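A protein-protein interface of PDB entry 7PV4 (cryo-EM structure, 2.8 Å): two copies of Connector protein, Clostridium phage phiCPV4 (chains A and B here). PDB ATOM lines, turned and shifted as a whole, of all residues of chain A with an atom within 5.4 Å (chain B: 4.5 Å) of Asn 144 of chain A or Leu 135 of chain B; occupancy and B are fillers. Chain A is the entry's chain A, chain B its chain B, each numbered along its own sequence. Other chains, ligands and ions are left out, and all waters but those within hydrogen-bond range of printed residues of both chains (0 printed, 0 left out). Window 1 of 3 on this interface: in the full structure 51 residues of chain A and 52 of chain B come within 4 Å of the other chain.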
ATOM      1  N   ILE A 139     -20.748  -4.486 -10.205  1.00  0.00           N
ATOM      2  CA  ILE A 139     -19.788  -3.669  -9.454  1.00  0.00           C
ATOM      3  C   ILE A 139     -18.619  -3.275 -10.356  1.00  0.00           C
ATOM      4  O   ILE A 139     -18.227  -2.117 -10.384  1.00  0.00           O
ATOM      5  CB  ILE A 139     -19.296  -4.373  -8.165  1.00  0.00           C
ATOM      6  CG1 ILE A 139     -20.447  -4.737  -7.215  1.00  0.00           C
ATOM      7  CG2 ILE A 139     -18.294  -3.487  -7.400  1.00  0.00           C
ATOM      8  CD1 ILE A 139     -20.052  -5.745  -6.135  1.00  0.00           C
ATOM      9  N   GLU A 140     -18.075  -4.202 -11.134  1.00  0.00           N
ATOM     10  CA  GLU A 140     -17.016  -3.910 -12.099  1.00  0.00           C
ATOM     11  C   GLU A 140     -17.419  -2.850 -13.116  1.00  0.00           C
ATOM     12  O   GLU A 140     -16.673  -1.906 -13.339  1.00  0.00           O
ATOM     13  CB  GLU A 140     -16.629  -5.180 -12.854  1.00  0.00           C
ATOM     14  CG  GLU A 140     -15.445  -5.901 -12.237  1.00  0.00           C
ATOM     15  CD  GLU A 140     -14.822  -6.954 -13.165  1.00  0.00           C
ATOM     16  OE1 GLU A 140     -15.178  -7.069 -14.341  1.00  0.00           O
ATOM     17  OE2 GLU A 140     -13.970  -7.724 -12.689  1.00  0.00           O
ATOM     18  N   MET A 141     -18.588  -2.981 -13.731  1.00  0.00           N
ATOM     19  CA  MET A 141     -19.085  -2.006 -14.682  1.00  0.00           C
ATOM     20  C   MET A 141     -19.201  -0.613 -14.058  1.00  0.00           C
ATOM     21  O   MET A 141     -18.763   0.367 -14.643  1.00  0.00           O
ATOM     22  CB  MET A 141     -20.409  -2.503 -15.250  1.00  0.00           C
ATOM     23  CG  MET A 141     -20.903  -1.613 -16.387  1.00  0.00           C
ATOM     24  SD  MET A 141     -22.471  -2.150 -17.075  1.00  0.00           S
ATOM     25  CE  MET A 141     -22.651  -0.887 -18.341  1.00  0.00           C
ATOM     26  N   THR A 142     -19.701  -0.528 -12.833  1.00  0.00           N
ATOM     27  CA  THR A 142     -19.827   0.712 -12.069  1.00  0.00           C
ATOM     28  C   THR A 142     -18.478   1.329 -11.709  1.00  0.00           C
ATOM     29  O   THR A 142     -18.336   2.538 -11.806  1.00  0.00           O
ATOM     30  CB  THR A 142     -20.667   0.475 -10.807  1.00  0.00           C
ATOM     31  OG1 THR A 142     -21.848  -0.192 -11.146  1.00  0.00           O
ATOM     32  CG2 THR A 142     -21.099   1.752 -10.104  1.00  0.00           C
ATOM     33  N   ILE A 143     -17.465   0.537 -11.361  1.00  0.00           N
ATOM     34  CA  ILE A 143     -16.083   0.987 -11.159  1.00  0.00           C
ATOM     35  C   ILE A 143     -15.546   1.648 -12.421  1.00  0.00           C
ATOM     36  O   ILE A 143     -15.037   2.759 -12.370  1.00  0.00           O
ATOM     37  CB  ILE A 143     -15.191  -0.191 -10.661  1.00  0.00           C
ATOM     38  CG1 ILE A 143     -15.431  -0.410  -9.159  1.00  0.00           C
ATOM     39  CG2 ILE A 143     -13.686  -0.016 -10.918  1.00  0.00           C
ATOM     40  CD1 ILE A 143     -14.825  -1.689  -8.590  1.00  0.00           C
ATOM     41  N   ASN A 144     -15.706   1.003 -13.566  1.00  0.00           N
ATOM     42  CA  ASN A 144     -15.210   1.471 -14.847  1.00  0.00           C
ATOM     43  C   ASN A 144     -15.907   2.736 -15.330  1.00  0.00           C
ATOM     44  O   ASN A 144     -15.239   3.637 -15.820  1.00  0.00           O
ATOM     45  CB  ASN A 144     -15.313   0.322 -15.857  1.00  0.00           C
ATOM     46  CG  ASN A 144     -14.179  -0.653 -15.659  1.00  0.00           C
ATOM     47  OD1 ASN A 144     -13.078  -0.413 -16.096  1.00  0.00           O
ATOM     48  ND2 ASN A 144     -14.373  -1.744 -14.966  1.00  0.00           N
ATOM     49  N   MET A 145     -17.220   2.842 -15.169  1.00  0.00           N
ATOM     50  CA  MET A 145     -17.963   4.046 -15.495  1.00  0.00           C
ATOM     51  C   MET A 145     -17.599   5.211 -14.578  1.00  0.00           C
ATOM     52  O   MET A 145     -17.358   6.310 -15.055  1.00  0.00           O
ATOM     53  CB  MET A 145     -19.464   3.746 -15.461  1.00  0.00           C
ATOM     54  CG  MET A 145     -19.889   2.894 -16.651  1.00  0.00           C
ATOM     55  SD  MET A 145     -21.652   2.510 -16.753  1.00  0.00           S
ATOM     56  CE  MET A 145     -22.372   4.093 -17.245  1.00  0.00           C
ATOM     57  N   ASN A 146     -17.484   4.988 -13.277  1.00  0.00           N
ATOM     58  CA  ASN A 146     -17.072   6.017 -12.344  1.00  0.00           C
ATOM     59  C   ASN A 146     -15.638   6.507 -12.587  1.00  0.00           C
ATOM     60  O   ASN A 146     -15.389   7.697 -12.480  1.00  0.00           O
ATOM     61  CB  ASN A 146     -17.274   5.504 -10.906  1.00  0.00           C
ATOM     62  CG  ASN A 146     -17.201   6.651  -9.932  1.00  0.00           C
ATOM     63  OD1 ASN A 146     -18.101   7.444  -9.812  1.00  0.00           O
ATOM     64  ND2 ASN A 146     -16.101   6.869  -9.281  1.00  0.00           N
ATOM     65  N   LEU A 147     -14.692   5.629 -12.921  1.00  0.00           N
ATOM     66  CA  LEU A 147     -13.328   6.005 -13.277  1.00  0.00           C
ATOM     67  C   LEU A 147     -13.301   6.883 -14.527  1.00  0.00           C
ATOM     68  O   LEU A 147     -12.673   7.930 -14.517  1.00  0.00           O
ATOM     69  CB  LEU A 147     -12.452   4.746 -13.425  1.00  0.00           C
ATOM     70  CG  LEU A 147     -10.990   4.997 -13.850  1.00  0.00           C
ATOM     71  CD1 LEU A 147     -10.157   5.720 -12.802  1.00  0.00           C
ATOM     72  CD2 LEU A 147     -10.314   3.675 -14.158  1.00  0.00           C
ATOM     73  N   ASP A 148     -14.024   6.526 -15.582  1.00  0.00           N
ATOM     74  CA  ASP A 148     -14.071   7.318 -16.806  1.00  0.00           C
ATOM     75  C   ASP A 148     -14.670   8.710 -16.588  1.00  0.00           C
ATOM     76  O   ASP A 148     -14.210   9.699 -17.144  1.00  0.00           O
ATOM     77  CB  ASP A 148     -14.881   6.544 -17.846  1.00  0.00           C
ATOM     78  CG  ASP A 148     -14.600   6.984 -19.277  1.00  0.00           C
ATOM     79  OD1 ASP A 148     -13.417   7.152 -19.626  1.00  0.00           O
ATOM     80  OD2 ASP A 148     -15.556   7.095 -20.070  1.00  0.00           O
ATOM     81  N   GLN A 149     -15.664   8.807 -15.714  1.00  0.00           N
ATOM     82  CA  GLN A 149     -16.309  10.055 -15.340  1.00  0.00           C
ATOM     83  C   GLN A 149     -15.398  11.029 -14.591  1.00  0.00           C
ATOM     84  O   GLN A 149     -15.611  12.232 -14.678  1.00  0.00           O
ATOM     85  CB  GLN A 149     -17.552   9.738 -14.516  1.00  0.00           C
ATOM     86  CG  GLN A 149     -18.700   9.224 -15.393  1.00  0.00           C
ATOM     87  CD  GLN A 149     -19.828   8.538 -14.630  1.00  0.00           C
ATOM     88  OE1 GLN A 149     -19.971   8.640 -13.427  1.00  0.00           O
ATOM     89  NE2 GLN A 149     -20.695   7.821 -15.302  1.00  0.00           N
ATOM     90  N   TYR B 131      -7.689  -8.267 -18.170  1.00  0.00           N
ATOM     91  CA  TYR B 131      -8.633  -7.325 -17.570  1.00  0.00           C
ATOM     92  C   TYR B 131      -7.930  -6.266 -16.709  1.00  0.00           C
ATOM     93  O   TYR B 131      -8.177  -5.072 -16.852  1.00  0.00           O
ATOM     94  CB  TYR B 131      -9.678  -8.070 -16.735  1.00  0.00           C
ATOM     95  CG  TYR B 131     -10.578  -7.126 -15.963  1.00  0.00           C
ATOM     96  CD1 TYR B 131     -11.537  -6.382 -16.663  1.00  0.00           C
ATOM     97  CD2 TYR B 131     -10.378  -6.884 -14.591  1.00  0.00           C
ATOM     98  CE1 TYR B 131     -12.248  -5.362 -16.015  1.00  0.00           C
ATOM     99  CE2 TYR B 131     -11.097  -5.874 -13.937  1.00  0.00           C
ATOM    100  CZ  TYR B 131     -12.020  -5.091 -14.658  1.00  0.00           C
ATOM    101  OH  TYR B 131     -12.709  -4.093 -14.050  1.00  0.00           O
ATOM    102  N   TYR B 132      -7.033  -6.681 -15.821  1.00  0.00           N
ATOM    103  CA  TYR B 132      -6.354  -5.768 -14.921  1.00  0.00           C
ATOM    104  C   TYR B 132      -5.338  -4.861 -15.628  1.00  0.00           C
ATOM    105  O   TYR B 132      -5.134  -3.739 -15.178  1.00  0.00           O
ATOM    106  CB  TYR B 132      -5.754  -6.547 -13.748  1.00  0.00           C
ATOM    107  CG  TYR B 132      -6.755  -6.777 -12.640  1.00  0.00           C
ATOM    108  CD1 TYR B 132      -7.099  -5.705 -11.801  1.00  0.00           C
ATOM    109  CD2 TYR B 132      -7.388  -8.020 -12.477  1.00  0.00           C
ATOM    110  CE1 TYR B 132      -8.084  -5.855 -10.811  1.00  0.00           C
ATOM    111  CE2 TYR B 132      -8.369  -8.177 -11.489  1.00  0.00           C
ATOM    112  CZ  TYR B 132      -8.725  -7.095 -10.667  1.00  0.00           C
ATOM    113  OH  TYR B 132      -9.701  -7.248  -9.754  1.00  0.00           O
ATOM    114  N   THR B 133      -4.749  -5.249 -16.761  1.00  0.00           N
ATOM    115  CA  THR B 133      -3.861  -4.351 -17.507  1.00  0.00           C
ATOM    116  C   THR B 133      -4.651  -3.271 -18.218  1.00  0.00           C
ATOM    117  O   THR B 133      -4.233  -2.117 -18.202  1.00  0.00           O
ATOM    118  CB  THR B 133      -2.940  -5.094 -18.488  1.00  0.00           C
ATOM    119  OG1 THR B 133      -3.636  -5.821 -19.461  1.00  0.00           O
ATOM    120  CG2 THR B 133      -2.015  -6.066 -17.773  1.00  0.00           C
ATOM    121  N   TYR B 134      -5.827  -3.595 -18.759  1.00  0.00           N
ATOM    122  CA  TYR B 134      -6.755  -2.596 -19.247  1.00  0.00           C
ATOM    123  C   TYR B 134      -7.108  -1.589 -18.143  1.00  0.00           C
ATOM    124  O   TYR B 134      -6.932  -0.397 -18.346  1.00  0.00           O
ATOM    125  CB  TYR B 134      -7.982  -3.282 -19.855  1.00  0.00           C
ATOM    126  CG  TYR B 134      -9.131  -2.329 -20.091  1.00  0.00           C
ATOM    127  CD1 TYR B 134      -9.114  -1.440 -21.186  1.00  0.00           C
ATOM    128  CD2 TYR B 134     -10.132  -2.221 -19.112  1.00  0.00           C
ATOM    129  CE1 TYR B 134     -10.085  -0.430 -21.284  1.00  0.00           C
ATOM    130  CE2 TYR B 134     -11.082  -1.200 -19.193  1.00  0.00           C
ATOM    131  CZ  TYR B 134     -11.060  -0.303 -20.279  1.00  0.00           C
ATOM    132  OH  TYR B 134     -11.993   0.675 -20.350  1.00  0.00           O
ATOM    133  N   LEU B 135      -7.488  -2.038 -16.951  1.00  0.00           N
ATOM    134  CA  LEU B 135      -7.836  -1.171 -15.833  1.00  0.00           C
ATOM    135  C   LEU B 135      -6.675  -0.276 -15.379  1.00  0.00           C
ATOM    136  O   LEU B 135      -6.844   0.931 -15.287  1.00  0.00           O
ATOM    137  CB  LEU B 135      -8.434  -2.047 -14.717  1.00  0.00           C
ATOM    138  CG  LEU B 135      -8.965  -1.309 -13.473  1.00  0.00           C
ATOM    139  CD1 LEU B 135     -10.070  -0.319 -13.806  1.00  0.00           C
ATOM    140  CD2 LEU B 135      -9.551  -2.314 -12.501  1.00  0.00           C
ATOM    141  N   MET B 136      -5.469  -0.808 -15.183  1.00  0.00           N
ATOM    142  CA  MET B 136      -4.312  -0.021 -14.756  1.00  0.00           C
ATOM    143  C   MET B 136      -3.870   1.015 -15.790  1.00  0.00           C
ATOM    144  O   MET B 136      -3.442   2.099 -15.410  1.00  0.00           O
ATOM    145  CB  MET B 136      -3.161  -0.947 -14.332  1.00  0.00           C
ATOM    146  CG  MET B 136      -3.499  -1.723 -13.054  1.00  0.00           C
ATOM    147  SD  MET B 136      -2.368  -3.080 -12.684  1.00  0.00           S
ATOM    148  CE  MET B 136      -3.322  -4.059 -11.521  1.00  0.00           C
ATOM    149  N   SER B 137      -4.052   0.754 -17.084  1.00  0.00           N
ATOM    150  CA  SER B 137      -3.822   1.746 -18.127  1.00  0.00           C
ATOM    151  C   SER B 137      -4.842   2.907 -18.109  1.00  0.00           C
ATOM    152  O   SER B 137      -4.489   4.043 -18.401  1.00  0.00           O
ATOM    153  CB  SER B 137      -3.771   1.044 -19.479  1.00  0.00           C
ATOM    154  OG  SER B 137      -5.050   0.715 -19.954  1.00  0.00           O
ATOM    155  N   GLN B 138      -6.085   2.675 -17.692  1.00  0.00           N
ATOM    156  CA  GLN B 138      -7.111   3.707 -17.526  1.00  0.00           C
ATOM    157  C   GLN B 138      -6.893   4.560 -16.279  1.00  0.00           C
ATOM    158  O   GLN B 138      -7.145   5.762 -16.309  1.00  0.00           O
ATOM    159  CB  GLN B 138      -8.504   3.067 -17.490  1.00  0.00           C
ATOM    160  CG  GLN B 138      -8.952   2.458 -18.822  1.00  0.00           C
ATOM    161  CD  GLN B 138      -9.000   3.454 -19.969  1.00  0.00           C
ATOM    162  OE1 GLN B 138      -9.465   4.569 -19.850  1.00  0.00           O
ATOM    163  NE2 GLN B 138      -8.510   3.120 -21.123  1.00  0.00           N
ATOM    164  N   ILE B 139      -6.381   3.977 -15.197  1.00  0.00           N
ATOM    165  CA  ILE B 139      -5.976   4.718 -13.998  1.00  0.00           C
ATOM    166  C   ILE B 139      -4.818   5.658 -14.331  1.00  0.00           C
ATOM    167  O   ILE B 139      -4.845   6.822 -13.957  1.00  0.00           O
ATOM    168  CB  ILE B 139      -5.622   3.780 -12.817  1.00  0.00           C
ATOM    169  CG1 ILE B 139      -6.785   2.856 -12.427  1.00  0.00           C
ATOM    170  CG2 ILE B 139      -5.205   4.591 -11.575  1.00  0.00           C
ATOM    171  CD1 ILE B 139      -6.364   1.683 -11.541  1.00  0.00           C
ATOM    172  N   CYS B 217      -6.050  -2.600  -6.807  1.00  0.00           N
ATOM    173  CA  CYS B 217      -6.222  -3.431  -7.999  1.00  0.00           C
ATOM    174  C   CYS B 217      -5.117  -4.464  -8.174  1.00  0.00           C
ATOM    175  O   CYS B 217      -5.385  -5.586  -8.590  1.00  0.00           O
ATOM    176  CB  CYS B 217      -6.297  -2.538  -9.243  1.00  0.00           C
ATOM    177  SG  CYS B 217      -7.848  -1.627  -9.270  1.00  0.00           S
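OH of Tyr 131 of chain B lies within hydrogen-bond range of ND2 of Asn 144 of chain A, at 3.0 Å.
The side-chain amide nitrogen (ND2) of Asn 144 of chain A lies within hydrogen-bond range of the backbone carbonyl oxygen (O) of Glu 140 of chain A, 2.8 Å away.
OG of Ser 137 of chain B sits at hydrogen-bond distance from O of Tyr 134 of chain B (2.7 Å).
Among the printed residues, pairs that only touch across the chains: Glu 140 of chain A with Tyr 131 of chain B, Asn 144 of chain A with Tyr 134 of chain B, Asn 144 of chain A with Leu 135 of chain B and Leu 147 of chain A with Gln 138 of chain B.
Printed residues of chain B within 4 Å of Glu 140 of chain A: Tyr 131 (3.6 Å).
Asn 144 of chain A touches just these residues of chain B: Tyr 131 (3.0 Å), Tyr 134 (3.8 Å) and Leu 135 (3.8 Å).
Printed residues of chain B within 4 Å of Leu 147 of chain A: Gln 138.
Asp 148 of chain A touches none of the printed residues of chain B.
Of the printed residues of chain A, Tyr 131 of chain B touches Glu 140 and Asn 144.
Printed residues of chain A within 4 Å of Tyr 134 of chain B: Asn 144.
Printed residues of chain A within 4 Å of Leu 135 of chain B: Asn 144.
Printed residues of chain A within 4 Å of Gln 138 of chain B: Leu 147 (3.8 Å).
The nearest printed residue of chain A that does not touch Tyr 134 of chain B is Asp 148 of chain A (6.7 Å).
Of the 11 printed residues of chain A, 3 touch a printed residue of chain B.
Printed residues of chain A that touch a printed residue of chain B: Glu 140, Asn 144 and Leu 147.
Hydrophobic or aromatic side chains of chain A within 4 Å of the printed part of chain B: Leu 147.
Along chain A the printed residues that touch a printed residue of chain B span positions 140 to 147.
Of the 10 printed residues of chain B, 4 touch a printed residue of chain A.
Printed residues of chain B that touch a printed residue of chain A: Tyr 131, Tyr 134, Leu 135 and Gln 138.
Hydrophobic or aromatic side chains of chain B within 4 Å of the printed part of chain A: Tyr 131, Tyr 134 and Leu 135.
Among the printed residues, 5 pairs touch across the chains.
Position printed for both chains: 139.
Of the 5 pairs that touch across the chains among the printed residues, none has its exchanged pair printed and touching as well.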
